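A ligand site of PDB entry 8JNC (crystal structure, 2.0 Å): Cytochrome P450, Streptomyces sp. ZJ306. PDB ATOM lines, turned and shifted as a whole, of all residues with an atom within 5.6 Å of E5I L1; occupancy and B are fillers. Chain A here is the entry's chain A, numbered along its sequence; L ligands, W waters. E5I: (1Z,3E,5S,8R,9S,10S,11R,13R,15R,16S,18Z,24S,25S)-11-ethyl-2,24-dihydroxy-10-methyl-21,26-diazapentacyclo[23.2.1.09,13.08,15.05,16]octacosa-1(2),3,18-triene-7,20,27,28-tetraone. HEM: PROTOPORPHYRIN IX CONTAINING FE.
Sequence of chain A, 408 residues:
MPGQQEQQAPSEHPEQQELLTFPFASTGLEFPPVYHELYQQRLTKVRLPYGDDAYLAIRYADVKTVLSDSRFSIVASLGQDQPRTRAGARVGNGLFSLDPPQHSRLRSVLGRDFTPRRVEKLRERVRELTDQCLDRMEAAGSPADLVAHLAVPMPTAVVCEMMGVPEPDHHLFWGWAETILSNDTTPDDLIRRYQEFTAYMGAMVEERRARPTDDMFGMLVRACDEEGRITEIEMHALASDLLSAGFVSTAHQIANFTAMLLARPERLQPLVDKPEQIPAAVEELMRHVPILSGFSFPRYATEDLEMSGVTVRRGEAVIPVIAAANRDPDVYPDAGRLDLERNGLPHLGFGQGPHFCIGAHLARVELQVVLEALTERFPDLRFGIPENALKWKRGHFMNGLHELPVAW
Gly 92 touches E5I L1 (CA to O37, 3.7 Å).
CE2 of Phe 96 touches C15 of E5I L1, 3.9 Å away.
Ile 180 touches E5I L1.
Leu 181 touches E5I L1.
Ser 240 touches E5I L1.
Ala 245 touches E5I L1.
Ser 249 touches E5I L1.
Ile 291 touches E5I L1 (CD1 to C34, 3.9 Å).
Leu 292 touches E5I L1.
Ser 296 touches E5I L1 (CB to O36, 3.3 Å).
CE1 of Phe 297 touches C21 of E5I L1, 3.6 Å away.
Phe 397 touches E5I L1 (CE2 to C20, 3.5 Å).
CE of Met 398 touches C30 of E5I L1, 3.4 Å away.
Hydrophobic or aromatic side chains within 4 Å of E5I L1: Phe 96, Ile 180, Leu 181, Ala 245, Ile 291, Leu 292, Phe 297, Phe 397 and Met 398.
18 residues have an atom within 4 Å of E5I L1: Arg 86, Arg 90, Val 91, Gly 92, Phe 96, Ile 180, Leu 181, Ser 240, Asp 241, Ser 244, Ala 245, Ser 249, Ile 291, Leu 292, Ser 296, Phe 297, Phe 397 and Met 398.
The nearest printed residue that does not touch E5I L1 is Ala 89 (4.2 Å).
The side-chain hydroxyl (OG) of Ser 240 sits at hydrogen-bond distance from the guanidinium group (NH2) of Arg 193.
The backbone carbonyl oxygen (O) of Ala 89 lies within hydrogen-bond range of the guanidinium group (NH2) of Arg 86 (3.3 Å).
NH1 of Arg 86 lies within hydrogen-bond range of O of Ile 180 (2.9 Å).
The side-chain hydroxyl of Ser 249 is in hydrogen-bond range of the backbone carbonyl oxygen of Ala 245 (2.7 Å).
O of Leu 181 sits at hydrogen-bond distance from N of Phe 397 (3.0 Å).
NE of Arg 86 is in hydrogen-bond range of O of Gly 88, at 2.8 Å.
OG of Ser 244 lies within hydrogen-bond range of O of Ser 240, 3.0 Å away.
N3 of E5I L1 sits at hydrogen-bond distance from O of Val 91, 3.2 Å away.
An oxygen (O8) of E5I L1 sits at hydrogen-bond distance from the guanidinium group (NH1) of Arg 90 (2.9 Å).
An oxygen (O25) of E5I L1 sits close to the side-chain hydroxyl of Ser 244 (3.2 Å).
A nitrogen (N12) of E5I L1 sits at hydrogen-bond distance from the side-chain carboxylate (OD1) of Asp 241 (2.8 Å).
O2A of HEM L2 lies within hydrogen-bond range of OG of Ser 296 (2.8 Å).
The guanidinium group (NH2) of Arg 86 sits at hydrogen-bond distance from an oxygen (O9) of E5I L1.
Water W3 lies within hydrogen-bond range of O37 of E5I L1 (2.5 Å), N of Asn 93 (2.8 Å) and N of Gly 94 (3.3 Å).
Water W2 lies within hydrogen-bond range of the side-chain carboxylate (OD1) of Asp 241 (2.7 Å), an oxygen (O26) of E5I L1 (2.8 Å) and the backbone NH (N) of Phe 96 (3.2 Å).
Water W5 lies within hydrogen-bond range of the side-chain carboxylate of Asp 241 (2.7 Å), the backbone carbonyl oxygen of Ala 237 (2.8 Å) and an oxygen (O37) of E5I L1 (3.3 Å).
Water W4 lies within hydrogen-bond range of the backbone NH of Gly 94, the backbone NH of Asn 93 and an oxygen (O37) of E5I L1.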
ATOM      1  N   ARG A  86      -5.603   7.689   5.783  1.00  0.00           N
ATOM      2  CA  ARG A  86      -5.506   6.370   6.402  1.00  0.00           C
ATOM      3  C   ARG A  86      -5.193   5.329   5.342  1.00  0.00           C
ATOM      4  O   ARG A  86      -5.810   5.313   4.273  1.00  0.00           O
ATOM      5  CB  ARG A  86      -6.809   6.007   7.129  1.00  0.00           C
ATOM      6  CG  ARG A  86      -6.661   4.940   8.209  1.00  0.00           C
ATOM      7  CD  ARG A  86      -8.017   4.483   8.801  1.00  0.00           C
ATOM      8  NE  ARG A  86      -8.881   3.836   7.822  1.00  0.00           N
ATOM      9  CZ  ARG A  86     -10.183   3.654   7.995  1.00  0.00           C
ATOM     10  NH1 ARG A  86     -10.795   4.038   9.115  1.00  0.00           N
ATOM     11  NH2 ARG A  86     -10.888   3.048   7.035  1.00  0.00           N
ATOM     12  N   GLY A  88      -5.839   2.211   5.015  1.00  0.00           N
ATOM     13  CA  GLY A  88      -7.014   1.482   4.592  1.00  0.00           C
ATOM     14  C   GLY A  88      -8.203   2.358   4.235  1.00  0.00           C
ATOM     15  O   GLY A  88      -8.686   3.109   5.080  1.00  0.00           O
ATOM     16  N   ALA A  89      -8.691   2.231   2.999  1.00  0.00           N
ATOM     17  CA  ALA A  89      -9.834   2.994   2.511  1.00  0.00           C
ATOM     18  C   ALA A  89     -11.043   2.832   3.416  1.00  0.00           C
ATOM     19  O   ALA A  89     -11.265   1.789   4.031  1.00  0.00           O
ATOM     20  N   ARG A  90     -11.832   3.894   3.503  1.00  0.00           N
ATOM     21  CA  ARG A  90     -12.911   3.966   4.477  1.00  0.00           C
ATOM     22  C   ARG A  90     -14.130   3.437   3.758  1.00  0.00           C
ATOM     23  O   ARG A  90     -14.741   4.153   2.969  1.00  0.00           O
ATOM     24  CB  ARG A  90     -13.130   5.391   4.966  1.00  0.00           C
ATOM     25  CG  ARG A  90     -11.865   6.137   5.390  1.00  0.00           C
ATOM     26  CD  ARG A  90     -12.281   7.497   5.936  1.00  0.00           C
ATOM     27  NE  ARG A  90     -11.157   8.259   6.424  1.00  0.00           N
ATOM     28  CZ  ARG A  90     -10.571   8.081   7.596  1.00  0.00           C
ATOM     29  NH1 ARG A  90     -11.029   7.213   8.485  1.00  0.00           N
ATOM     30  NH2 ARG A  90      -9.487   8.796   7.875  1.00  0.00           N
ATOM     31  N   VAL A  91     -14.485   2.185   4.019  1.00  0.00           N
ATOM     32  CA  VAL A  91     -15.551   1.543   3.267  1.00  0.00           C
ATOM     33  C   VAL A  91     -16.410   0.672   4.179  1.00  0.00           C
ATOM     34  O   VAL A  91     -15.913   0.039   5.116  1.00  0.00           O
ATOM     35  CB  VAL A  91     -14.974   0.723   2.102  1.00  0.00           C
ATOM     36  CG1 VAL A  91     -14.128   1.629   1.216  1.00  0.00           C
ATOM     37  CG2 VAL A  91     -14.167  -0.486   2.616  1.00  0.00           C
ATOM     38  N   GLY A  92     -17.699   0.656   3.907  1.00  0.00           N
ATOM     39  CA  GLY A  92     -18.593  -0.135   4.727  1.00  0.00           C
ATOM     40  C   GLY A  92     -19.992   0.062   4.245  1.00  0.00           C
ATOM     41  O   GLY A  92     -20.201   0.546   3.136  1.00  0.00           O
ATOM     42  N   ASN A  93     -20.960  -0.285   5.105  1.00  0.00           N
ATOM     43  CA  ASN A  93     -22.380  -0.347   4.757  1.00  0.00           C
ATOM     44  C   ASN A  93     -23.231   0.679   5.500  1.00  0.00           C
ATOM     45  O   ASN A  93     -24.468   0.576   5.459  1.00  0.00           O
ATOM     46  CB  ASN A  93     -22.924  -1.745   5.061  1.00  0.00           C
ATOM     47  CG  ASN A  93     -22.397  -2.783   4.096  1.00  0.00           C
ATOM     48  OD1 ASN A  93     -22.980  -3.014   3.035  1.00  0.00           O
ATOM     49  ND2 ASN A  93     -21.296  -3.429   4.458  1.00  0.00           N
ATOM     50  N   GLY A  94     -22.596   1.636   6.170  1.00  0.00           N
ATOM     51  CA  GLY A  94     -23.270   2.647   6.965  1.00  0.00           C
ATOM     52  C   GLY A  94     -23.466   3.970   6.243  1.00  0.00           C
ATOM     53  O   GLY A  94     -23.389   4.058   5.009  1.00  0.00           O
ATOM     54  N   PHE A  96     -22.010   6.912   5.817  1.00  0.00           N
ATOM     55  CA  PHE A  96     -20.963   7.546   5.019  1.00  0.00           C
ATOM     56  C   PHE A  96     -20.674   6.801   3.706  1.00  0.00           C
ATOM     57  O   PHE A  96     -19.922   7.289   2.856  1.00  0.00           O
ATOM     58  CB  PHE A  96     -19.674   7.639   5.843  1.00  0.00           C
ATOM     59  CG  PHE A  96     -19.605   8.836   6.772  1.00  0.00           C
ATOM     60  CD1 PHE A  96     -19.626  10.128   6.282  1.00  0.00           C
ATOM     61  CD2 PHE A  96     -19.464   8.660   8.127  1.00  0.00           C
ATOM     62  CE1 PHE A  96     -19.533  11.248   7.150  1.00  0.00           C
ATOM     63  CE2 PHE A  96     -19.352   9.765   8.990  1.00  0.00           C
ATOM     64  CZ  PHE A  96     -19.389  11.053   8.494  1.00  0.00           C
ATOM     65  N   ILE A 180     -10.407   3.001  14.086  1.00  0.00           N
ATOM     66  CA  ILE A 180     -11.035   3.689  12.954  1.00  0.00           C
ATOM     67  C   ILE A 180     -10.370   5.031  12.709  1.00  0.00           C
ATOM     68  O   ILE A 180     -10.034   5.370  11.578  1.00  0.00           O
ATOM     69  CB  ILE A 180     -12.532   3.883  13.192  1.00  0.00           C
ATOM     70  CG1 ILE A 180     -13.240   2.596  12.912  1.00  0.00           C
ATOM     71  CG2 ILE A 180     -13.034   5.009  12.329  1.00  0.00           C
ATOM     72  CD1 ILE A 180     -13.226   2.159  11.443  1.00  0.00           C
ATOM     73  N   LEU A 181     -10.174   5.807  13.771  1.00  0.00           N
ATOM     74  CA  LEU A 181      -9.706   7.175  13.651  1.00  0.00           C
ATOM     75  C   LEU A 181      -8.173   7.289  13.507  1.00  0.00           C
ATOM     76  O   LEU A 181      -7.660   8.380  13.257  1.00  0.00           O
ATOM     77  CB  LEU A 181     -10.196   7.951  14.876  1.00  0.00           C
ATOM     78  CG  LEU A 181     -11.724   7.881  15.005  1.00  0.00           C
ATOM     79  CD1 LEU A 181     -12.309   8.392  16.305  1.00  0.00           C
ATOM     80  CD2 LEU A 181     -12.420   8.620  13.843  1.00  0.00           C
ATOM     81  N   LEU A 190      -8.339  -3.099  10.319  1.00  0.00           N
ATOM     82  CA  LEU A 190      -9.754  -2.854  10.116  1.00  0.00           C
ATOM     83  C   LEU A 190     -10.516  -4.164  10.121  1.00  0.00           C
ATOM     84  O   LEU A 190     -11.661  -4.214  10.588  1.00  0.00           O
ATOM     85  CB  LEU A 190      -9.991  -2.106   8.812  1.00  0.00           C
ATOM     86  CG  LEU A 190      -9.552  -0.647   8.810  1.00  0.00           C
ATOM     87  CD1 LEU A 190      -9.489  -0.116   7.408  1.00  0.00           C
ATOM     88  CD2 LEU A 190     -10.494   0.150   9.677  1.00  0.00           C
ATOM     89  N   ARG A 193     -10.783  -5.258  13.821  1.00  0.00           N
ATOM     90  CA  ARG A 193     -11.870  -4.476  14.407  1.00  0.00           C
ATOM     91  C   ARG A 193     -13.222  -4.994  13.934  1.00  0.00           C
ATOM     92  O   ARG A 193     -14.115  -5.239  14.751  1.00  0.00           O
ATOM     93  CB  ARG A 193     -11.745  -2.990  14.047  1.00  0.00           C
ATOM     94  CG  ARG A 193     -12.849  -2.171  14.673  1.00  0.00           C
ATOM     95  CD  ARG A 193     -13.060  -0.795  14.058  1.00  0.00           C
ATOM     96  NE  ARG A 193     -14.356  -0.267  14.476  1.00  0.00           N
ATOM     97  CZ  ARG A 193     -15.514  -0.642  13.946  1.00  0.00           C
ATOM     98  NH1 ARG A 193     -15.567  -1.425  12.882  1.00  0.00           N
ATOM     99  NH2 ARG A 193     -16.647  -0.173  14.473  1.00  0.00           N
ATOM    100  N   ALA A 237     -24.386  -1.803  10.844  1.00  0.00           N
ATOM    101  CA  ALA A 237     -23.728  -0.616  10.316  1.00  0.00           C
ATOM    102  C   ALA A 237     -24.148   0.632  11.076  1.00  0.00           C
ATOM    103  O   ALA A 237     -23.318   1.483  11.420  1.00  0.00           O
ATOM    104  CB  ALA A 237     -24.014  -0.476   8.824  1.00  0.00           C
ATOM    105  N   SER A 240     -22.555   0.680  14.420  1.00  0.00           N
ATOM    106  CA  SER A 240     -21.127   0.945  14.290  1.00  0.00           C
ATOM    107  C   SER A 240     -20.862   2.430  14.018  1.00  0.00           C
ATOM    108  O   SER A 240     -19.921   3.009  14.583  1.00  0.00           O
ATOM    109  CB  SER A 240     -20.568   0.048  13.186  1.00  0.00           C
ATOM    110  OG  SER A 240     -19.194   0.222  13.029  1.00  0.00           O
ATOM    111  N   ASP A 241     -21.668   3.051  13.160  1.00  0.00           N
ATOM    112  CA  ASP A 241     -21.537   4.486  12.913  1.00  0.00           C
ATOM    113  C   ASP A 241     -21.672   5.262  14.213  1.00  0.00           C
ATOM    114  O   ASP A 241     -20.868   6.147  14.531  1.00  0.00           O
ATOM    115  CB  ASP A 241     -22.608   4.976  11.925  1.00  0.00           C
ATOM    116  CG  ASP A 241     -22.313   4.591  10.460  1.00  0.00           C
ATOM    117  OD1 ASP A 241     -21.158   4.273  10.107  1.00  0.00           O
ATOM    118  OD2 ASP A 241     -23.302   4.594   9.678  1.00  0.00           O
ATOM    119  N   SER A 244     -18.815   4.631  16.705  1.00  0.00           N
ATOM    120  CA  SER A 244     -17.541   5.180  16.271  1.00  0.00           C
ATOM    121  C   SER A 244     -17.521   6.695  16.367  1.00  0.00           C
ATOM    122  O   SER A 244     -16.504   7.288  16.720  1.00  0.00           O
ATOM    123  CB  SER A 244     -17.229   4.796  14.829  1.00  0.00           C
ATOM    124  OG  SER A 244     -16.973   3.437  14.683  1.00  0.00           O
ATOM    125  N   ALA A 245     -18.618   7.318  16.010  1.00  0.00           N
ATOM    126  CA  ALA A 245     -18.644   8.756  15.885  1.00  0.00           C
ATOM    127  C   ALA A 245     -19.062   9.436  17.166  1.00  0.00           C
ATOM    128  O   ALA A 245     -18.823  10.621  17.329  1.00  0.00           O
ATOM    129  CB  ALA A 245     -19.607   9.166  14.763  1.00  0.00           C
ATOM    130  N   SER A 249     -15.606  12.142  19.397  1.00  0.00           N
ATOM    131  CA  SER A 249     -15.824  13.491  18.878  1.00  0.00           C
ATOM    132  C   SER A 249     -15.967  14.502  20.005  1.00  0.00           C
ATOM    133  O   SER A 249     -15.157  15.437  20.138  1.00  0.00           O
ATOM    134  CB  SER A 249     -17.110  13.492  18.022  1.00  0.00           C
ATOM    135  OG  SER A 249     -18.174  12.834  18.709  1.00  0.00           O
ATOM    136  N   GLN A 253     -13.624  17.593  21.686  1.00  0.00           N
ATOM    137  CA  GLN A 253     -14.110  18.989  21.677  1.00  0.00           C
ATOM    138  C   GLN A 253     -14.290  19.563  23.090  1.00  0.00           C
ATOM    139  O   GLN A 253     -14.071  20.779  23.286  1.00  0.00           O
ATOM    140  CB  GLN A 253     -15.427  19.106  20.902  1.00  0.00           C
ATOM    141  CG  GLN A 253     -15.232  19.075  19.429  1.00  0.00           C
ATOM    142  CD  GLN A 253     -14.542  20.326  18.847  1.00  0.00           C
ATOM    143  OE1 GLN A 253     -13.421  20.646  19.202  1.00  0.00           O
ATOM    144  NE2 GLN A 253     -15.195  20.979  17.905  1.00  0.00           N
ATOM    145  N   ILE A 291     -11.076  21.014  14.192  1.00  0.00           N
ATOM    146  CA  ILE A 291     -11.080  19.767  14.896  1.00  0.00           C
ATOM    147  C   ILE A 291     -10.398  18.657  14.108  1.00  0.00           C
ATOM    148  O   ILE A 291      -9.825  17.716  14.685  1.00  0.00           O
ATOM    149  CB  ILE A 291     -12.516  19.369  15.288  1.00  0.00           C
ATOM    150  CG1 ILE A 291     -12.380  18.089  16.056  1.00  0.00           C
ATOM    151  CG2 ILE A 291     -13.352  19.088  14.050  1.00  0.00           C
ATOM    152  CD1 ILE A 291     -13.192  18.015  17.330  1.00  0.00           C
ATOM    153  N   LEU A 292     -10.390  18.751  12.775  1.00  0.00           N
ATOM    154  CA  LEU A 292      -9.820  17.727  11.909  1.00  0.00           C
ATOM    155  C   LEU A 292      -8.340  17.999  11.621  1.00  0.00           C
ATOM    156  O   LEU A 292      -7.953  19.097  11.217  1.00  0.00           O
ATOM    157  CB  LEU A 292     -10.594  17.580  10.599  1.00  0.00           C
ATOM    158  CG  LEU A 292     -12.083  17.237  10.789  1.00  0.00           C
ATOM    159  CD1 LEU A 292     -12.764  17.006   9.464  1.00  0.00           C
ATOM    160  CD2 LEU A 292     -12.255  16.010  11.685  1.00  0.00           C
ATOM    161  N   PHE A 295      -9.034  15.667   6.865  1.00  0.00           N
ATOM    162  CA  PHE A 295     -10.354  15.931   6.301  1.00  0.00           C
ATOM    163  C   PHE A 295     -11.190  14.694   6.549  1.00  0.00           C
ATOM    164  O   PHE A 295     -10.746  13.723   7.173  1.00  0.00           O
ATOM    165  CB  PHE A 295     -10.256  16.269   4.818  1.00  0.00           C
ATOM    166  CG  PHE A 295      -9.652  15.145   3.939  1.00  0.00           C
ATOM    167  CD1 PHE A 295      -8.286  14.919   3.902  1.00  0.00           C
ATOM    168  CD2 PHE A 295     -10.471  14.380   3.126  1.00  0.00           C
ATOM    169  CE1 PHE A 295      -7.748  13.945   3.068  1.00  0.00           C
ATOM    170  CE2 PHE A 295      -9.938  13.371   2.297  1.00  0.00           C
ATOM    171  CZ  PHE A 295      -8.588  13.167   2.272  1.00  0.00           C
ATOM    172  N   SER A 296     -12.426  14.728   6.063  1.00  0.00           N
ATOM    173  CA  SER A 296     -13.411  13.686   6.391  1.00  0.00           C
ATOM    174  C   SER A 296     -13.522  12.677   5.246  1.00  0.00           C
ATOM    175  O   SER A 296     -12.819  11.648   5.234  1.00  0.00           O
ATOM    176  CB  SER A 296     -14.770  14.319   6.702  1.00  0.00           C
ATOM    177  OG  SER A 296     -15.154  15.250   5.684  1.00  0.00           O
ATOM    178  N   PHE A 297     -14.454  12.929   4.330  1.00  0.00           N
ATOM    179  CA  PHE A 297     -14.653  12.137   3.146  1.00  0.00           C
ATOM    180  C   PHE A 297     -14.588  13.057   1.925  1.00  0.00           C
ATOM    181  O   PHE A 297     -15.235  14.098   1.911  1.00  0.00           O
ATOM    182  CB  PHE A 297     -15.991  11.408   3.154  1.00  0.00           C
ATOM    183  CG  PHE A 297     -16.035  10.234   4.092  1.00  0.00           C
ATOM    184  CD1 PHE A 297     -16.212  10.398   5.438  1.00  0.00           C
ATOM    185  CD2 PHE A 297     -15.921   8.943   3.588  1.00  0.00           C
ATOM    186  CE1 PHE A 297     -16.269   9.282   6.312  1.00  0.00           C
ATOM    187  CE2 PHE A 297     -15.958   7.843   4.429  1.00  0.00           C
ATOM    188  CZ  PHE A 297     -16.139   8.017   5.796  1.00  0.00           C
ATOM    189  N   ILE A 322     -13.889  21.884   6.050  1.00  0.00           N
ATOM    190  CA  ILE A 322     -14.834  22.631   6.894  1.00  0.00           C
ATOM    191  C   ILE A 322     -14.114  23.677   7.737  1.00  0.00           C
ATOM    192  O   ILE A 322     -14.666  24.759   7.978  1.00  0.00           O
ATOM    193  CB  ILE A 322     -15.677  21.695   7.779  1.00  0.00           C
ATOM    194  CG1 ILE A 322     -14.795  20.833   8.660  1.00  0.00           C
ATOM    195  CG2 ILE A 322     -16.629  20.799   6.913  1.00  0.00           C
ATOM    196  CD1 ILE A 322     -15.606  20.055   9.737  1.00  0.00           C
ATOM    197  N   PHE A 397      -6.839  11.266  13.476  1.00  0.00           N
ATOM    198  CA  PHE A 397      -7.772  11.933  12.580  1.00  0.00           C
ATOM    199  C   PHE A 397      -8.150  13.320  13.105  1.00  0.00           C
ATOM    200  O   PHE A 397      -8.321  14.269  12.333  1.00  0.00           O
ATOM    201  CB  PHE A 397      -8.996  11.028  12.443  1.00  0.00           C
ATOM    202  CG  PHE A 397      -9.972  11.472  11.473  1.00  0.00           C
ATOM    203  CD1 PHE A 397      -9.684  11.439  10.115  1.00  0.00           C
ATOM    204  CD2 PHE A 397     -11.206  11.896  11.874  1.00  0.00           C
ATOM    205  CE1 PHE A 397     -10.609  11.832   9.206  1.00  0.00           C
ATOM    206  CE2 PHE A 397     -12.152  12.308  10.953  1.00  0.00           C
ATOM    207  CZ  PHE A 397     -11.858  12.284   9.627  1.00  0.00           C
ATOM    208  N   MET A 398      -8.269  13.457  14.434  1.00  0.00           N
ATOM    209  CA  MET A 398      -8.637  14.717  15.072  1.00  0.00           C
ATOM    210  C   MET A 398      -7.504  15.425  15.814  1.00  0.00           C
ATOM    211  O   MET A 398      -6.549  14.809  16.298  1.00  0.00           O
ATOM    212  CB  MET A 398      -9.769  14.505  16.072  1.00  0.00           C
ATOM    213  CG  MET A 398     -11.069  14.031  15.503  1.00  0.00           C
ATOM    214  SD  MET A 398     -11.912  13.077  16.764  1.00  0.00           S
ATOM    215  CE  MET A 398     -13.324  12.537  15.829  1.00  0.00           C
HETATM  216  C1  E5I L   1     -15.125   4.243   7.796  1.00  0.00           C
HETATM  217  C10 E5I L   1     -17.299   2.054  10.080  1.00  0.00           C
HETATM  218  C11 E5I L   1     -18.214   2.467  11.210  1.00  0.00           C
HETATM  219  C13 E5I L   1     -17.691   4.841  11.438  1.00  0.00           C
HETATM  220  C14 E5I L   1     -18.220   6.222  11.274  1.00  0.00           C
HETATM  221  C15 E5I L   1     -17.656   7.393  11.518  1.00  0.00           C
HETATM  222  C16 E5I L   1     -16.298   7.610  12.113  1.00  0.00           C
HETATM  223  C17 E5I L   1     -15.602   8.832  11.501  1.00  0.00           C
HETATM  224  C18 E5I L   1     -16.394  10.120  11.768  1.00  0.00           C
HETATM  225  C19 E5I L   1     -15.623  11.343  11.233  1.00  0.00           C
HETATM  226  C2  E5I L   1     -14.541   2.896   7.665  1.00  0.00           C
HETATM  227  C20 E5I L   1     -15.286  11.157   9.754  1.00  0.00           C
HETATM  228  C21 E5I L   1     -14.576   9.866   9.470  1.00  0.00           C
HETATM  229  C22 E5I L   1     -15.385   8.687   9.989  1.00  0.00           C
HETATM  230  C23 E5I L   1     -14.587   7.484   9.615  1.00  0.00           C
HETATM  231  C24 E5I L   1     -15.084   6.454   8.976  1.00  0.00           C
HETATM  232  C27 E5I L   1     -16.624  10.460  13.229  1.00  0.00           C
HETATM  233  C28 E5I L   1     -17.029  11.942  13.190  1.00  0.00           C
HETATM  234  C29 E5I L   1     -16.494  12.452  11.836  1.00  0.00           C
HETATM  235  C30 E5I L   1     -16.305  12.798  14.234  1.00  0.00           C
HETATM  236  C31 E5I L   1     -16.334  14.156  13.533  1.00  0.00           C
HETATM  237  C32 E5I L   1     -15.838  13.808  12.135  1.00  0.00           C
HETATM  238  C33 E5I L   1     -15.288  15.099  14.110  1.00  0.00           C
HETATM  239  C34 E5I L   1     -15.521  15.515  15.517  1.00  0.00           C
HETATM  240  C35 E5I L   1     -16.122  14.840  11.053  1.00  0.00           C
HETATM  241  C4  E5I L   1     -16.895   2.673   7.651  1.00  0.00           C
HETATM  242  C5  E5I L   1     -16.581   4.117   7.764  1.00  0.00           C
HETATM  243  C6  E5I L   1     -17.860   2.071   8.662  1.00  0.00           C
HETATM  244  C7  E5I L   1     -14.454   5.264   8.454  1.00  0.00           C
HETATM  245  N12 E5I L   1     -18.576   3.870  11.149  1.00  0.00           N
HETATM  246  N3  E5I L   1     -15.593   2.078   7.598  1.00  0.00           N
HETATM  247  O25 E5I L   1     -16.535   4.589  11.770  1.00  0.00           O
HETATM  248  O26 E5I L   1     -17.430   4.978   7.788  1.00  0.00           O
HETATM  249  O36 E5I L   1     -15.596  11.955   8.908  1.00  0.00           O
HETATM  250  O37 E5I L   1     -18.248   0.745   8.280  1.00  0.00           O
HETATM  251  O8  E5I L   1     -13.152   5.210   8.567  1.00  0.00           O
HETATM  252  O9  E5I L   1     -13.375   2.564   7.599  1.00  0.00           O
HETATM  253  CHA HEM L   2     -21.174  13.278  10.674  1.00  0.00           C
HETATM  254  CHB HEM L   2     -18.939  16.666  13.285  1.00  0.00           C
HETATM  255  CHC HEM L   2     -20.528  14.636  17.373  1.00  0.00           C
HETATM  256  CHD HEM L   2     -22.479  11.077  14.817  1.00  0.00           C
HETATM  257  C1A HEM L   2     -20.508  14.422  11.026  1.00  0.00           C
HETATM  258  C2A HEM L   2     -19.969  15.412  10.116  1.00  0.00           C
HETATM  259  C3A HEM L   2     -19.348  16.336  10.833  1.00  0.00           C
HETATM  260  C4A HEM L   2     -19.466  15.982  12.226  1.00  0.00           C
HETATM  261  CMA HEM L   2     -18.643  17.604  10.302  1.00  0.00           C
HETATM  262  CAA HEM L   2     -20.107  15.405   8.595  1.00  0.00           C
HETATM  263  CBA HEM L   2     -18.815  14.939   7.900  1.00  0.00           C
HETATM  264  CGA HEM L   2     -18.924  14.892   6.368  1.00  0.00           C
HETATM  265  O1A HEM L   2     -20.008  15.168   5.774  1.00  0.00           O
HETATM  266  O2A HEM L   2     -17.909  14.602   5.666  1.00  0.00           O
HETATM  267  C1B HEM L   2     -19.115  16.406  14.621  1.00  0.00           C
HETATM  268  C2B HEM L   2     -18.562  17.140  15.766  1.00  0.00           C
HETATM  269  C3B HEM L   2     -19.018  16.544  16.874  1.00  0.00           C
HETATM  270  C4B HEM L   2     -19.861  15.449  16.495  1.00  0.00           C
HETATM  271  CMB HEM L   2     -17.602  18.354  15.674  1.00  0.00           C
HETATM  272  CAB HEM L   2     -18.764  16.887  18.346  1.00  0.00           C
HETATM  273  CBB HEM L   2     -18.376  18.106  18.687  1.00  0.00           C
HETATM  274  C1C HEM L   2     -21.283  13.564  17.033  1.00  0.00           C
HETATM  275  C2C HEM L   2     -22.124  12.782  17.928  1.00  0.00           C
HETATM  276  C3C HEM L   2     -22.642  11.794  17.187  1.00  0.00           C
HETATM  277  C4C HEM L   2     -22.154  11.936  15.838  1.00  0.00           C
HETATM  278  CMC HEM L   2     -22.344  13.119  19.417  1.00  0.00           C
HETATM  279  CAC HEM L   2     -23.631  10.695  17.609  1.00  0.00           C
HETATM  280  CBC HEM L   2     -23.811  10.352  18.897  1.00  0.00           C
HETATM  281  C1D HEM L   2     -22.280  11.300  13.483  1.00  0.00           C
HETATM  282  C2D HEM L   2     -22.715  10.444  12.378  1.00  0.00           C
HETATM  283  C3D HEM L   2     -22.328  11.090  11.185  1.00  0.00           C
HETATM  284  C4D HEM L   2     -21.674  12.326  11.553  1.00  0.00           C
HETATM  285  CMD HEM L   2     -23.446   9.064  12.549  1.00  0.00           C
HETATM  286  CAD HEM L   2     -22.552  10.603   9.715  1.00  0.00           C
HETATM  287  CBD HEM L   2     -23.958  11.094   9.351  1.00  0.00           C
HETATM  288  CGD HEM L   2     -24.355  10.739   7.956  1.00  0.00           C
HETATM  289  O1D HEM L   2     -25.581  10.741   7.705  1.00  0.00           O
HETATM  290  O2D HEM L   2     -23.509  10.456   7.098  1.00  0.00           O
HETATM  291  NA  HEM L   2     -20.153  14.773  12.312  1.00  0.00           N
HETATM  292  NB  HEM L   2     -19.888  15.394  15.114  1.00  0.00           N
HETATM  293  NC  HEM L   2     -21.330  13.025  15.784  1.00  0.00           N
HETATM  294  ND  HEM L   2     -21.678  12.414  12.938  1.00  0.00           N
HETATM  295 FE   HEM L   2     -21.041  14.038  14.047  1.00  0.00          FE
HETATM  296  O   HOH W   1     -17.401  -1.590   8.601  1.00  0.00           O
HETATM  297  O   HOH W   2     -20.233   4.971   7.720  1.00  0.00           O
HETATM  298  O   HOH W   3     -20.518  -0.308   7.832  1.00  0.00           O
HETATM  299  O   HOH W   4     -19.925   2.731   6.075  1.00  0.00           O
HETATM  300  O   HOH W   5     -21.141   1.624   9.633  1.00  0.00           O
